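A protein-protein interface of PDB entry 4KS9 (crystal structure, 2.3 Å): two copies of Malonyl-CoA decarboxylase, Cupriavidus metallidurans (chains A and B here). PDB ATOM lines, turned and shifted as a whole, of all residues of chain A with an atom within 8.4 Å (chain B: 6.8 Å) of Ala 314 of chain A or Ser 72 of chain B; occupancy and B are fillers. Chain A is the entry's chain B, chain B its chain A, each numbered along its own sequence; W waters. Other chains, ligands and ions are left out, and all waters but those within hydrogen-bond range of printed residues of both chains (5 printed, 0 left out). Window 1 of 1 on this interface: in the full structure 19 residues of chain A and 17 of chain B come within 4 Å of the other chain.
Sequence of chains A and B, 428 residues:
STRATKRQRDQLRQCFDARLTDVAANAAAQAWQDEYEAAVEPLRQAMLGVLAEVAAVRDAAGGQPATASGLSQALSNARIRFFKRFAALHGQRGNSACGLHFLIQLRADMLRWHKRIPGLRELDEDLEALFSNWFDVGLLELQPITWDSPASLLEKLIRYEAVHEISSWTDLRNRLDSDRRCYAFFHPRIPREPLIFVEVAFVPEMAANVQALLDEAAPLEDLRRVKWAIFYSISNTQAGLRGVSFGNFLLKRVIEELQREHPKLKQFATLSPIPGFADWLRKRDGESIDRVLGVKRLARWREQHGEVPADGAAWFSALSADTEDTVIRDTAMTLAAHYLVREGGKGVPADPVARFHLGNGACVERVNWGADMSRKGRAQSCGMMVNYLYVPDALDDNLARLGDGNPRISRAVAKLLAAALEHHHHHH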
ATOM      1  N   LEU A 281      15.181   3.985 -24.518  1.00  0.00           N
ATOM      2  CA  LEU A 281      14.282   4.732 -23.653  1.00  0.00           C
ATOM      3  C   LEU A 281      13.765   3.923 -22.468  1.00  0.00           C
ATOM      4  O   LEU A 281      13.793   4.398 -21.329  1.00  0.00           O
ATOM      5  CB  LEU A 281      13.100   5.290 -24.456  1.00  0.00           C
ATOM      6  CG  LEU A 281      12.157   6.199 -23.655  1.00  0.00           C
ATOM      7  CD1 LEU A 281      12.947   7.380 -23.060  1.00  0.00           C
ATOM      8  CD2 LEU A 281      11.027   6.694 -24.542  1.00  0.00           C
ATOM      9  N   ARG A 282      13.306   2.702 -22.720  1.00  0.00           N
ATOM     10  CA  ARG A 282      12.780   1.911 -21.627  1.00  0.00           C
ATOM     11  C   ARG A 282      13.836   1.414 -20.641  1.00  0.00           C
ATOM     12  O   ARG A 282      13.503   0.761 -19.659  1.00  0.00           O
ATOM     13  CB  ARG A 282      11.912   0.752 -22.148  1.00  0.00           C
ATOM     14  CG  ARG A 282      12.523  -0.118 -23.219  1.00  0.00           C
ATOM     15  CD  ARG A 282      11.699  -1.401 -23.390  1.00  0.00           C
ATOM     16  NE  ARG A 282      10.290  -1.136 -23.685  1.00  0.00           N
ATOM     17  CZ  ARG A 282       9.792  -1.031 -24.911  1.00  0.00           C
ATOM     18  NH1 ARG A 282       8.500  -0.786 -25.087  1.00  0.00           N
ATOM     19  NH2 ARG A 282      10.584  -1.185 -25.964  1.00  0.00           N
ATOM     20  N   LYS A 283      15.100   1.738 -20.888  1.00  0.00           N
ATOM     21  CA  LYS A 283      16.170   1.350 -19.973  1.00  0.00           C
ATOM     22  C   LYS A 283      16.603   2.526 -19.087  1.00  0.00           C
ATOM     23  O   LYS A 283      17.487   2.381 -18.227  1.00  0.00           O
ATOM     24  CB  LYS A 283      17.390   0.841 -20.742  1.00  0.00           C
ATOM     25  CG  LYS A 283      17.234  -0.562 -21.306  1.00  0.00           C
ATOM     26  CD  LYS A 283      18.467  -0.960 -22.098  1.00  0.00           C
ATOM     27  CE  LYS A 283      18.359  -2.385 -22.615  1.00  0.00           C
ATOM     28  NZ  LYS A 283      19.572  -2.778 -23.392  1.00  0.00           N
ATOM     29  N   ARG A 284      15.979   3.684 -19.300  1.00  0.00           N
ATOM     30  CA  ARG A 284      16.302   4.898 -18.545  1.00  0.00           C
ATOM     31  C   ARG A 284      15.352   5.100 -17.374  1.00  0.00           C
ATOM     32  O   ARG A 284      14.159   4.790 -17.465  1.00  0.00           O
ATOM     33  CB  ARG A 284      16.208   6.131 -19.448  1.00  0.00           C
ATOM     34  CG  ARG A 284      17.043   6.069 -20.720  1.00  0.00           C
ATOM     35  CD  ARG A 284      18.446   6.611 -20.524  1.00  0.00           C
ATOM     36  NE  ARG A 284      19.296   5.744 -19.714  1.00  0.00           N
ATOM     37  CZ  ARG A 284      19.690   4.522 -20.068  1.00  0.00           C
ATOM     38  NH1 ARG A 284      19.303   4.000 -21.229  1.00  0.00           N
ATOM     39  NH2 ARG A 284      20.499   3.834 -19.267  1.00  0.00           N
ATOM     40  N   GLY A 286      13.522   7.672 -14.407  1.00  0.00           N
ATOM     41  CA  GLY A 286      12.892   8.979 -14.502  1.00  0.00           C
ATOM     42  C   GLY A 286      13.876  10.136 -14.461  1.00  0.00           C
ATOM     43  O   GLY A 286      13.795  11.086 -15.245  1.00  0.00           O
ATOM     44  N   TRP A 301       4.706  19.565 -20.056  1.00  0.00           N
ATOM     45  CA  TRP A 301       4.123  18.236 -20.032  1.00  0.00           C
ATOM     46  C   TRP A 301       3.082  18.079 -18.922  1.00  0.00           C
ATOM     47  O   TRP A 301       1.997  17.521 -19.139  1.00  0.00           O
ATOM     48  CB  TRP A 301       5.216  17.183 -19.856  1.00  0.00           C
ATOM     49  CG  TRP A 301       4.645  15.812 -19.692  1.00  0.00           C
ATOM     50  CD1 TRP A 301       4.163  15.255 -18.541  1.00  0.00           C
ATOM     51  CD2 TRP A 301       4.402  14.858 -20.731  1.00  0.00           C
ATOM     52  NE1 TRP A 301       3.632  14.015 -18.797  1.00  0.00           N
ATOM     53  CE2 TRP A 301       3.761  13.744 -20.134  1.00  0.00           C
ATOM     54  CE3 TRP A 301       4.664  14.830 -22.109  1.00  0.00           C
ATOM     55  CZ2 TRP A 301       3.378  12.620 -20.867  1.00  0.00           C
ATOM     56  CZ3 TRP A 301       4.286  13.703 -22.841  1.00  0.00           C
ATOM     57  CH2 TRP A 301       3.650  12.621 -22.216  1.00  0.00           C
ATOM     58  N   GLU A 307       0.481  13.906 -14.735  1.00  0.00           N
ATOM     59  CA  GLU A 307       1.592  13.069 -14.274  1.00  0.00           C
ATOM     60  C   GLU A 307       2.716  12.878 -15.279  1.00  0.00           C
ATOM     61  O   GLU A 307       2.475  12.699 -16.470  1.00  0.00           O
ATOM     62  CB  GLU A 307       1.085  11.681 -13.891  1.00  0.00           C
ATOM     63  CG  GLU A 307       0.365  11.593 -12.568  1.00  0.00           C
ATOM     64  CD  GLU A 307      -0.046  10.160 -12.230  1.00  0.00           C
ATOM     65  OE1 GLU A 307       0.554   9.201 -12.793  1.00  0.00           O
ATOM     66  OE2 GLU A 307      -0.958   9.998 -11.387  1.00  0.00           O
ATOM     67  N   VAL A 308       3.942  12.898 -14.778  1.00  0.00           N
ATOM     68  CA  VAL A 308       5.119  12.678 -15.594  1.00  0.00           C
ATOM     69  C   VAL A 308       5.367  11.171 -15.535  1.00  0.00           C
ATOM     70  O   VAL A 308       5.378  10.589 -14.455  1.00  0.00           O
ATOM     71  CB  VAL A 308       6.360  13.390 -15.000  1.00  0.00           C
ATOM     72  CG1 VAL A 308       7.591  13.112 -15.870  1.00  0.00           C
ATOM     73  CG2 VAL A 308       6.105  14.890 -14.880  1.00  0.00           C
ATOM     74  N   PRO A 309       5.546  10.512 -16.690  1.00  0.00           N
ATOM     75  CA  PRO A 309       5.796   9.069 -16.642  1.00  0.00           C
ATOM     76  C   PRO A 309       6.893   8.774 -15.619  1.00  0.00           C
ATOM     77  O   PRO A 309       7.888   9.484 -15.570  1.00  0.00           O
ATOM     78  CB  PRO A 309       6.232   8.748 -18.072  1.00  0.00           C
ATOM     79  CG  PRO A 309       5.381   9.675 -18.875  1.00  0.00           C
ATOM     80  CD  PRO A 309       5.451  10.984 -18.083  1.00  0.00           C
ATOM     81  N   ALA A 310       6.697   7.730 -14.814  1.00  0.00           N
ATOM     82  CA  ALA A 310       7.649   7.355 -13.777  1.00  0.00           C
ATOM     83  C   ALA A 310       9.066   7.052 -14.267  1.00  0.00           C
ATOM     84  O   ALA A 310      10.045   7.385 -13.586  1.00  0.00           O
ATOM     85  CB  ALA A 310       7.102   6.168 -12.980  1.00  0.00           C
ATOM     86  N   ASP A 311       9.178   6.419 -15.432  1.00  0.00           N
ATOM     87  CA  ASP A 311      10.484   6.079 -16.009  1.00  0.00           C
ATOM     88  C   ASP A 311      10.452   5.964 -17.539  1.00  0.00           C
ATOM     89  O   ASP A 311       9.437   6.221 -18.173  1.00  0.00           O
ATOM     90  CB  ASP A 311      11.014   4.764 -15.422  1.00  0.00           C
ATOM     91  CG  ASP A 311      10.025   3.626 -15.547  1.00  0.00           C
ATOM     92  OD1 ASP A 311       9.318   3.553 -16.574  1.00  0.00           O
ATOM     93  OD2 ASP A 311       9.966   2.793 -14.616  1.00  0.00           O
ATOM     94  N   GLY A 312      11.578   5.569 -18.113  1.00  0.00           N
ATOM     95  CA  GLY A 312      11.674   5.436 -19.548  1.00  0.00           C
ATOM     96  C   GLY A 312      10.616   4.539 -20.148  1.00  0.00           C
ATOM     97  O   GLY A 312       9.989   4.901 -21.133  1.00  0.00           O
ATOM     98  N   ALA A 313      10.409   3.371 -19.556  1.00  0.00           N
ATOM     99  CA  ALA A 313       9.412   2.447 -20.079  1.00  0.00           C
ATOM    100  C   ALA A 313       8.044   3.121 -20.102  1.00  0.00           C
ATOM    101  O   ALA A 313       7.299   3.031 -21.091  1.00  0.00           O
ATOM    102  CB  ALA A 313       9.366   1.169 -19.222  1.00  0.00           C
ATOM    103  N   ALA A 314       7.716   3.808 -19.016  1.00  0.00           N
ATOM    104  CA  ALA A 314       6.429   4.470 -18.939  1.00  0.00           C
ATOM    105  C   ALA A 314       6.393   5.618 -19.941  1.00  0.00           C
ATOM    106  O   ALA A 314       5.333   5.947 -20.472  1.00  0.00           O
ATOM    107  CB  ALA A 314       6.167   4.972 -17.519  1.00  0.00           C
ATOM    108  N   TRP A 315       7.556   6.210 -20.208  1.00  0.00           N
ATOM    109  CA  TRP A 315       7.637   7.303 -21.164  1.00  0.00           C
ATOM    110  C   TRP A 315       7.298   6.787 -22.573  1.00  0.00           C
ATOM    111  O   TRP A 315       6.551   7.413 -23.307  1.00  0.00           O
ATOM    112  CB  TRP A 315       9.038   7.923 -21.151  1.00  0.00           C
ATOM    113  CG  TRP A 315       9.177   9.150 -20.253  1.00  0.00           C
ATOM    114  CD1 TRP A 315       9.949   9.263 -19.131  1.00  0.00           C
ATOM    115  CD2 TRP A 315       8.545  10.421 -20.432  1.00  0.00           C
ATOM    116  NE1 TRP A 315       9.841  10.517 -18.603  1.00  0.00           N
ATOM    117  CE2 TRP A 315       8.989  11.257 -19.379  1.00  0.00           C
ATOM    118  CE3 TRP A 315       7.649  10.941 -21.381  1.00  0.00           C
ATOM    119  CZ2 TRP A 315       8.571  12.594 -19.246  1.00  0.00           C
ATOM    120  CZ3 TRP A 315       7.229  12.273 -21.247  1.00  0.00           C
ATOM    121  CH2 TRP A 315       7.697  13.081 -20.183  1.00  0.00           C
ATOM    122  N   PHE A 316       7.835   5.630 -22.935  1.00  0.00           N
ATOM    123  CA  PHE A 316       7.559   5.076 -24.243  1.00  0.00           C
ATOM    124  C   PHE A 316       6.065   4.839 -24.434  1.00  0.00           C
ATOM    125  O   PHE A 316       5.517   5.130 -25.494  1.00  0.00           O
ATOM    126  CB  PHE A 316       8.321   3.770 -24.434  1.00  0.00           C
ATOM    127  CG  PHE A 316       8.301   3.271 -25.841  1.00  0.00           C
ATOM    128  CD1 PHE A 316       8.985   3.953 -26.843  1.00  0.00           C
ATOM    129  CD2 PHE A 316       7.568   2.140 -26.183  1.00  0.00           C
ATOM    130  CE1 PHE A 316       8.935   3.517 -28.163  1.00  0.00           C
ATOM    131  CE2 PHE A 316       7.515   1.701 -27.503  1.00  0.00           C
ATOM    132  CZ  PHE A 316       8.200   2.393 -28.491  1.00  0.00           C
ATOM    133  N   SER A 317       5.398   4.332 -23.401  1.00  0.00           N
ATOM    134  CA  SER A 317       3.965   4.058 -23.477  1.00  0.00           C
ATOM    135  C   SER A 317       3.108   5.320 -23.561  1.00  0.00           C
ATOM    136  O   SER A 317       2.019   5.317 -24.163  1.00  0.00           O
ATOM    137  CB  SER A 317       3.530   3.223 -22.273  1.00  0.00           C
ATOM    138  OG  SER A 317       4.290   2.034 -22.211  1.00  0.00           O
ATOM    139  N   ALA A 318       3.603   6.393 -22.952  1.00  0.00           N
ATOM    140  CA  ALA A 318       2.895   7.661 -22.954  1.00  0.00           C
ATOM    141  C   ALA A 318       3.083   8.368 -24.301  1.00  0.00           C
ATOM    142  O   ALA A 318       2.176   9.034 -24.792  1.00  0.00           O
ATOM    143  CB  ALA A 318       3.410   8.540 -21.808  1.00  0.00           C
ATOM    144  N   LEU A 319       4.261   8.199 -24.895  1.00  0.00           N
ATOM    145  CA  LEU A 319       4.596   8.824 -26.171  1.00  0.00           C
ATOM    146  C   LEU A 319       4.013   8.097 -27.391  1.00  0.00           C
ATOM    147  O   LEU A 319       4.133   8.574 -28.523  1.00  0.00           O
ATOM    148  CB  LEU A 319       6.120   8.918 -26.307  1.00  0.00           C
ATOM    149  CG  LEU A 319       6.824   9.831 -25.291  1.00  0.00           C
ATOM    150  CD1 LEU A 319       8.324   9.797 -25.527  1.00  0.00           C
ATOM    151  CD2 LEU A 319       6.302  11.255 -25.420  1.00  0.00           C
ATOM    152  N   SER A 320       3.382   6.948 -27.153  1.00  0.00           N
ATOM    153  CA  SER A 320       2.791   6.147 -28.221  1.00  0.00           C
ATOM    154  C   SER A 320       1.263   6.208 -28.171  1.00  0.00           C
ATOM    155  O   SER A 320       0.587   5.738 -29.082  1.00  0.00           O
ATOM    156  CB  SER A 320       3.238   4.688 -28.081  1.00  0.00           C
ATOM    157  OG  SER A 320       4.648   4.571 -27.960  1.00  0.00           O
ATOM    158  N   ALA A 321       0.733   6.816 -27.113  1.00  0.00           N
ATOM    159  CA  ALA A 321      -0.708   6.915 -26.891  1.00  0.00           C
ATOM    160  C   ALA A 321      -1.503   7.929 -27.715  1.00  0.00           C
ATOM    161  O   ALA A 321      -2.736   7.873 -27.737  1.00  0.00           O
ATOM    162  CB  ALA A 321      -0.970   7.160 -25.404  1.00  0.00           C
ATOM    163  N   THR B  67      -4.188   8.794 -16.087  1.00  0.00           N
ATOM    164  CA  THR B  67      -2.831   9.184 -15.739  1.00  0.00           C
ATOM    165  C   THR B  67      -1.784   8.309 -16.431  1.00  0.00           C
ATOM    166  O   THR B  67      -2.108   7.272 -17.016  1.00  0.00           O
ATOM    167  CB  THR B  67      -2.623   9.134 -14.207  1.00  0.00           C
ATOM    168  OG1 THR B  67      -2.873   7.810 -13.722  1.00  0.00           O
ATOM    169  CG2 THR B  67      -3.582  10.095 -13.517  1.00  0.00           C
ATOM    170  N   ALA B  68      -0.528   8.742 -16.368  1.00  0.00           N
ATOM    171  CA  ALA B  68       0.575   8.011 -16.983  1.00  0.00           C
ATOM    172  C   ALA B  68       0.846   6.709 -16.229  1.00  0.00           C
ATOM    173  O   ALA B  68       1.159   5.683 -16.832  1.00  0.00           O
ATOM    174  CB  ALA B  68       1.827   8.880 -17.001  1.00  0.00           C
ATOM    175  N   SER B  69       0.734   6.763 -14.904  1.00  0.00           N
ATOM    176  CA  SER B  69       0.955   5.580 -14.067  1.00  0.00           C
ATOM    177  C   SER B  69      -0.187   4.591 -14.294  1.00  0.00           C
ATOM    178  O   SER B  69       0.002   3.381 -14.198  1.00  0.00           O
ATOM    179  CB  SER B  69       1.017   5.964 -12.582  1.00  0.00           C
ATOM    180  OG  SER B  69      -0.267   6.264 -12.065  1.00  0.00           O
ATOM    181  N   GLY B  70      -1.366   5.134 -14.594  1.00  0.00           N
ATOM    182  CA  GLY B  70      -2.547   4.327 -14.845  1.00  0.00           C
ATOM    183  C   GLY B  70      -2.536   3.670 -16.214  1.00  0.00           C
ATOM    184  O   GLY B  70      -3.227   2.676 -16.429  1.00  0.00           O
ATOM    185  N   LEU B  71      -1.759   4.230 -17.141  1.00  0.00           N
ATOM    186  CA  LEU B  71      -1.653   3.681 -18.484  1.00  0.00           C
ATOM    187  C   LEU B  71      -0.760   2.449 -18.428  1.00  0.00           C
ATOM    188  O   LEU B  71      -1.142   1.383 -18.905  1.00  0.00           O
ATOM    189  CB  LEU B  71      -1.047   4.703 -19.449  1.00  0.00           C
ATOM    190  CG  LEU B  71      -0.918   4.188 -20.887  1.00  0.00           C
ATOM    191  CD1 LEU B  71      -2.315   3.917 -21.451  1.00  0.00           C
ATOM    192  CD2 LEU B  71      -0.169   5.201 -21.745  1.00  0.00           C
ATOM    193  N   SER B  72       0.429   2.609 -17.847  1.00  0.00           N
ATOM    194  CA  SER B  72       1.377   1.504 -17.710  1.00  0.00           C
ATOM    195  C   SER B  72       0.713   0.305 -17.029  1.00  0.00           C
ATOM    196  O   SER B  72       0.869  -0.831 -17.467  1.00  0.00           O
ATOM    197  CB  SER B  72       2.600   1.935 -16.888  1.00  0.00           C
ATOM    198  OG  SER B  72       3.349   2.938 -17.552  1.00  0.00           O
ATOM    199  N   GLN B  73      -0.032   0.572 -15.961  1.00  0.00           N
ATOM    200  CA  GLN B  73      -0.724  -0.476 -15.209  1.00  0.00           C
ATOM    201  C   GLN B  73      -1.826  -1.143 -16.042  1.00  0.00           C
ATOM    202  O   GLN B  73      -1.993  -2.371 -16.015  1.00  0.00           O
ATOM    203  CB  GLN B  73      -1.334   0.113 -13.927  1.00  0.00           C
ATOM    204  CG  GLN B  73      -1.820  -0.925 -12.912  1.00  0.00           C
ATOM    205  CD  GLN B  73      -0.719  -1.885 -12.467  1.00  0.00           C
ATOM    206  OE1 GLN B  73       0.359  -1.464 -12.041  1.00  0.00           O
ATOM    207  NE2 GLN B  73      -0.993  -3.180 -12.559  1.00  0.00           N
ATOM    208  N   ALA B  74      -2.579  -0.324 -16.771  1.00  0.00           N
ATOM    209  CA  ALA B  74      -3.657  -0.822 -17.607  1.00  0.00           C
ATOM    210  C   ALA B  74      -3.101  -1.656 -18.752  1.00  0.00           C
ATOM    211  O   ALA B  74      -3.734  -2.605 -19.196  1.00  0.00           O
ATOM    212  CB  ALA B  74      -4.481   0.343 -18.151  1.00  0.00           C
ATOM    213  N   LEU B  75      -1.920  -1.286 -19.231  1.00  0.00           N
ATOM    214  CA  LEU B  75      -1.280  -2.004 -20.316  1.00  0.00           C
ATOM    215  C   LEU B  75      -0.711  -3.313 -19.781  1.00  0.00           C
ATOM    216  O   LEU B  75      -0.756  -4.345 -20.453  1.00  0.00           O
ATOM    217  CB  LEU B  75      -0.178  -1.144 -20.935  1.00  0.00           C
ATOM    218  CG  LEU B  75      -0.694   0.078 -21.709  1.00  0.00           C
ATOM    219  CD1 LEU B  75       0.467   0.980 -22.120  1.00  0.00           C
ATOM    220  CD2 LEU B  75      -1.466  -0.388 -22.936  1.00  0.00           C
ATOM    221  N   SER B  76      -0.180  -3.270 -18.568  1.00  0.00           N
ATOM    222  CA  SER B  76       0.365  -4.469 -17.953  1.00  0.00           C
ATOM    223  C   SER B  76      -0.776  -5.446 -17.661  1.00  0.00           C
ATOM    224  O   SER B  76      -0.685  -6.628 -17.995  1.00  0.00           O
ATOM    225  CB  SER B  76       1.089  -4.126 -16.651  1.00  0.00           C
ATOM    226  OG  SER B  76       1.658  -5.291 -16.075  1.00  0.00           O
ATOM    227  N   ASN B  77      -1.851  -4.937 -17.056  1.00  0.00           N
ATOM    228  CA  ASN B  77      -3.014  -5.753 -16.712  1.00  0.00           C
ATOM    229  C   ASN B  77      -3.716  -6.400 -17.914  1.00  0.00           C
ATOM    230  O   ASN B  77      -4.345  -7.452 -17.767  1.00  0.00           O
ATOM    231  CB  ASN B  77      -4.062  -4.927 -15.941  1.00  0.00           C
ATOM    232  CG  ASN B  77      -3.635  -4.592 -14.511  1.00  0.00           C
ATOM    233  OD1 ASN B  77      -2.713  -5.192 -13.956  1.00  0.00           O
ATOM    234  ND2 ASN B  77      -4.329  -3.637 -13.904  1.00  0.00           N
ATOM    235  N   ARG B  79      -2.152  -7.278 -20.905  1.00  0.00           N
ATOM    236  CA  ARG B  79      -1.263  -8.292 -21.443  1.00  0.00           C
ATOM    237  C   ARG B  79      -1.389  -9.530 -20.559  1.00  0.00           C
ATOM    238  O   ARG B  79      -1.464 -10.646 -21.048  1.00  0.00           O
ATOM    239  CB  ARG B  79       0.200  -7.805 -21.432  1.00  0.00           C
ATOM    240  CG  ARG B  79       0.549  -6.749 -22.480  1.00  0.00           C
ATOM    241  CD  ARG B  79       2.060  -6.600 -22.629  1.00  0.00           C
ATOM    242  NE  ARG B  79       2.665  -6.046 -21.422  1.00  0.00           N
ATOM    243  CZ  ARG B  79       2.609  -4.761 -21.084  1.00  0.00           C
ATOM    244  NH1 ARG B  79       1.982  -3.892 -21.870  1.00  0.00           N
ATOM    245  NH2 ARG B  79       3.161  -4.349 -19.949  1.00  0.00           N
ATOM    246  N   GLU B 122       7.695  -6.625 -23.906  1.00  0.00           N
ATOM    247  CA  GLU B 122       6.823  -6.579 -22.737  1.00  0.00           C
ATOM    248  C   GLU B 122       5.953  -7.831 -22.634  1.00  0.00           C
ATOM    249  O   GLU B 122       5.752  -8.356 -21.541  1.00  0.00           O
ATOM    250  CB  GLU B 122       5.965  -5.304 -22.779  1.00  0.00           C
ATOM    251  CG  GLU B 122       6.812  -4.025 -22.806  1.00  0.00           C
ATOM    252  CD  GLU B 122       6.008  -2.757 -23.078  1.00  0.00           C
ATOM    253  OE1 GLU B 122       5.162  -2.388 -22.237  1.00  0.00           O
ATOM    254  OE2 GLU B 122       6.225  -2.126 -24.138  1.00  0.00           O
HETATM  255  O   HOH W   1       2.670   5.586 -19.756  1.00  0.00           O
HETATM  256  O   HOH W   2       0.086  12.008 -17.416  1.00  0.00           O
HETATM  257  O   HOH W   3       4.904   1.185 -18.881  1.00  0.00           O
HETATM  258  O   HOH W   4       6.926   0.686 -22.646  1.00  0.00           O
HETATM  259  O   HOH W   5       3.431   8.216 -13.370  1.00  0.00           O
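OE2 of Glu 122 of chain B is in salt-bridge range of NH1 of Arg 282 of chain A (2.8 Å). The side-chain hydroxyl of Ser 69 of chain B is in hydrogen-bond range of the side-chain carboxylate of Glu 307 of chain A (3.1 Å).
The indole nitrogen (NE1) of Trp 301 of chain A sits at hydrogen-bond distance from the backbone carbonyl oxygen (O) of Glu 307 of chain A (2.9 Å). The guanidinium group (NH1) of Arg 79 of chain B lies within salt-bridge range of the side-chain carboxylate (OE1) of Glu 122 of chain B, 3.5 Å away. The backbone carbonyl oxygen (O) of Leu 75 of chain B is in hydrogen-bond range of the guanidinium group (NH1) of Arg 79 of chain B (3.1 Å). The side-chain hydroxyl of Ser 69 of chain B is in hydrogen-bond range of the side-chain hydroxyl of Thr 67 of chain B (3.5 Å). The side-chain carboxylate of Asp 311 of chain A sits at hydrogen-bond distance from the backbone NH of Ala 314 of chain A, at 2.9 Å. OG of Ser 317 of chain A lies within hydrogen-bond range of O of Ala 313 of chain A, 3.4 Å away.
Among the printed residues, pairs that only touch across the chains: Glu 307 of chain A with Thr 67 of chain B, Glu 307 of chain A with Ala 68 of chain B, Pro 309 of chain A with Ala 68 of chain B, Ala 314 of chain A with Ser 72 of chain B, Ser 317 of chain A with Leu 71 of chain B and Ser 317 of chain A with Leu 75 of chain B.
Printed residues of chain B within 4 Å of Arg 282 of chain A: Glu 122. Of chain B, only Ser 72 (3.5 Å) comes within 4 Å of Ala 314 of chain A. Of the printed residues of chain B, Ser 317 of chain A touches Leu 71 (3.3 Å) and Leu 75 (3.8 Å). Of the printed residues of chain A, Ala 68 of chain B touches Glu 307 (3.8 Å) and Pro 309 (3.99 Å). Ser 72 of chain B touches just one residue of chain A: Ala 314. Arg 79 of chain B touches none of the printed residues of chain A. Printed residues of chain A within 4 Å of Glu 122 of chain B: Arg 282 (2.8 Å). The nearest residue of chain A that does not touch Ser 72 of chain B is Ser 317 of chain A (4.7 Å).
Printed residues of chain A that touch a printed residue of chain B: Arg 282, Glu 307, Pro 309, Ala 314 and Ser 317. Hydrophobic or aromatic side chains of chain A that line the printed part of chain B: Ala 314. Among the printed residues, Asp or Glu carboxylates within 4 Å of a Lys or Arg side-chain nitrogen of the other chain: Arg 282 of chain A with Glu 122 of chain B (2.8 Å).
No position is printed for both chains. Of the 8 pairs that touch across the chains among the printed residues, none has its exchanged pair printed and touching as well.
Water W2 lies within hydrogen-bond range of O of Glu 307 of chain A (2.7 Å) and N of Ala 68 of chain B (3.5 Å). Water W3 bridges OG of Ser 72 of chain B (2.7 Å) and OG of Ser 317 of chain A (3.5 Å). Water W1 lies within hydrogen-bond range of the backbone carbonyl oxygen of Ala 314 of chain A (2.8 Å), the backbone carbonyl oxygen of Ala 68 of chain B (3.3 Å) and the backbone NH of Ala 318 of chain A (3.4 Å). Water W4 lies within hydrogen-bond range of O of Ala 313 of chain A, OG of Ser 317 of chain A, NH1 of Arg 282 of chain A and OE2 of Glu 122 of chain B. Water W5 lies within hydrogen-bond range of OE1 of Glu 307 of chain A (3.1 Å), O of Val 308 of chain A (3.3 Å) and N of Ser 69 of chain B (3.4 Å).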
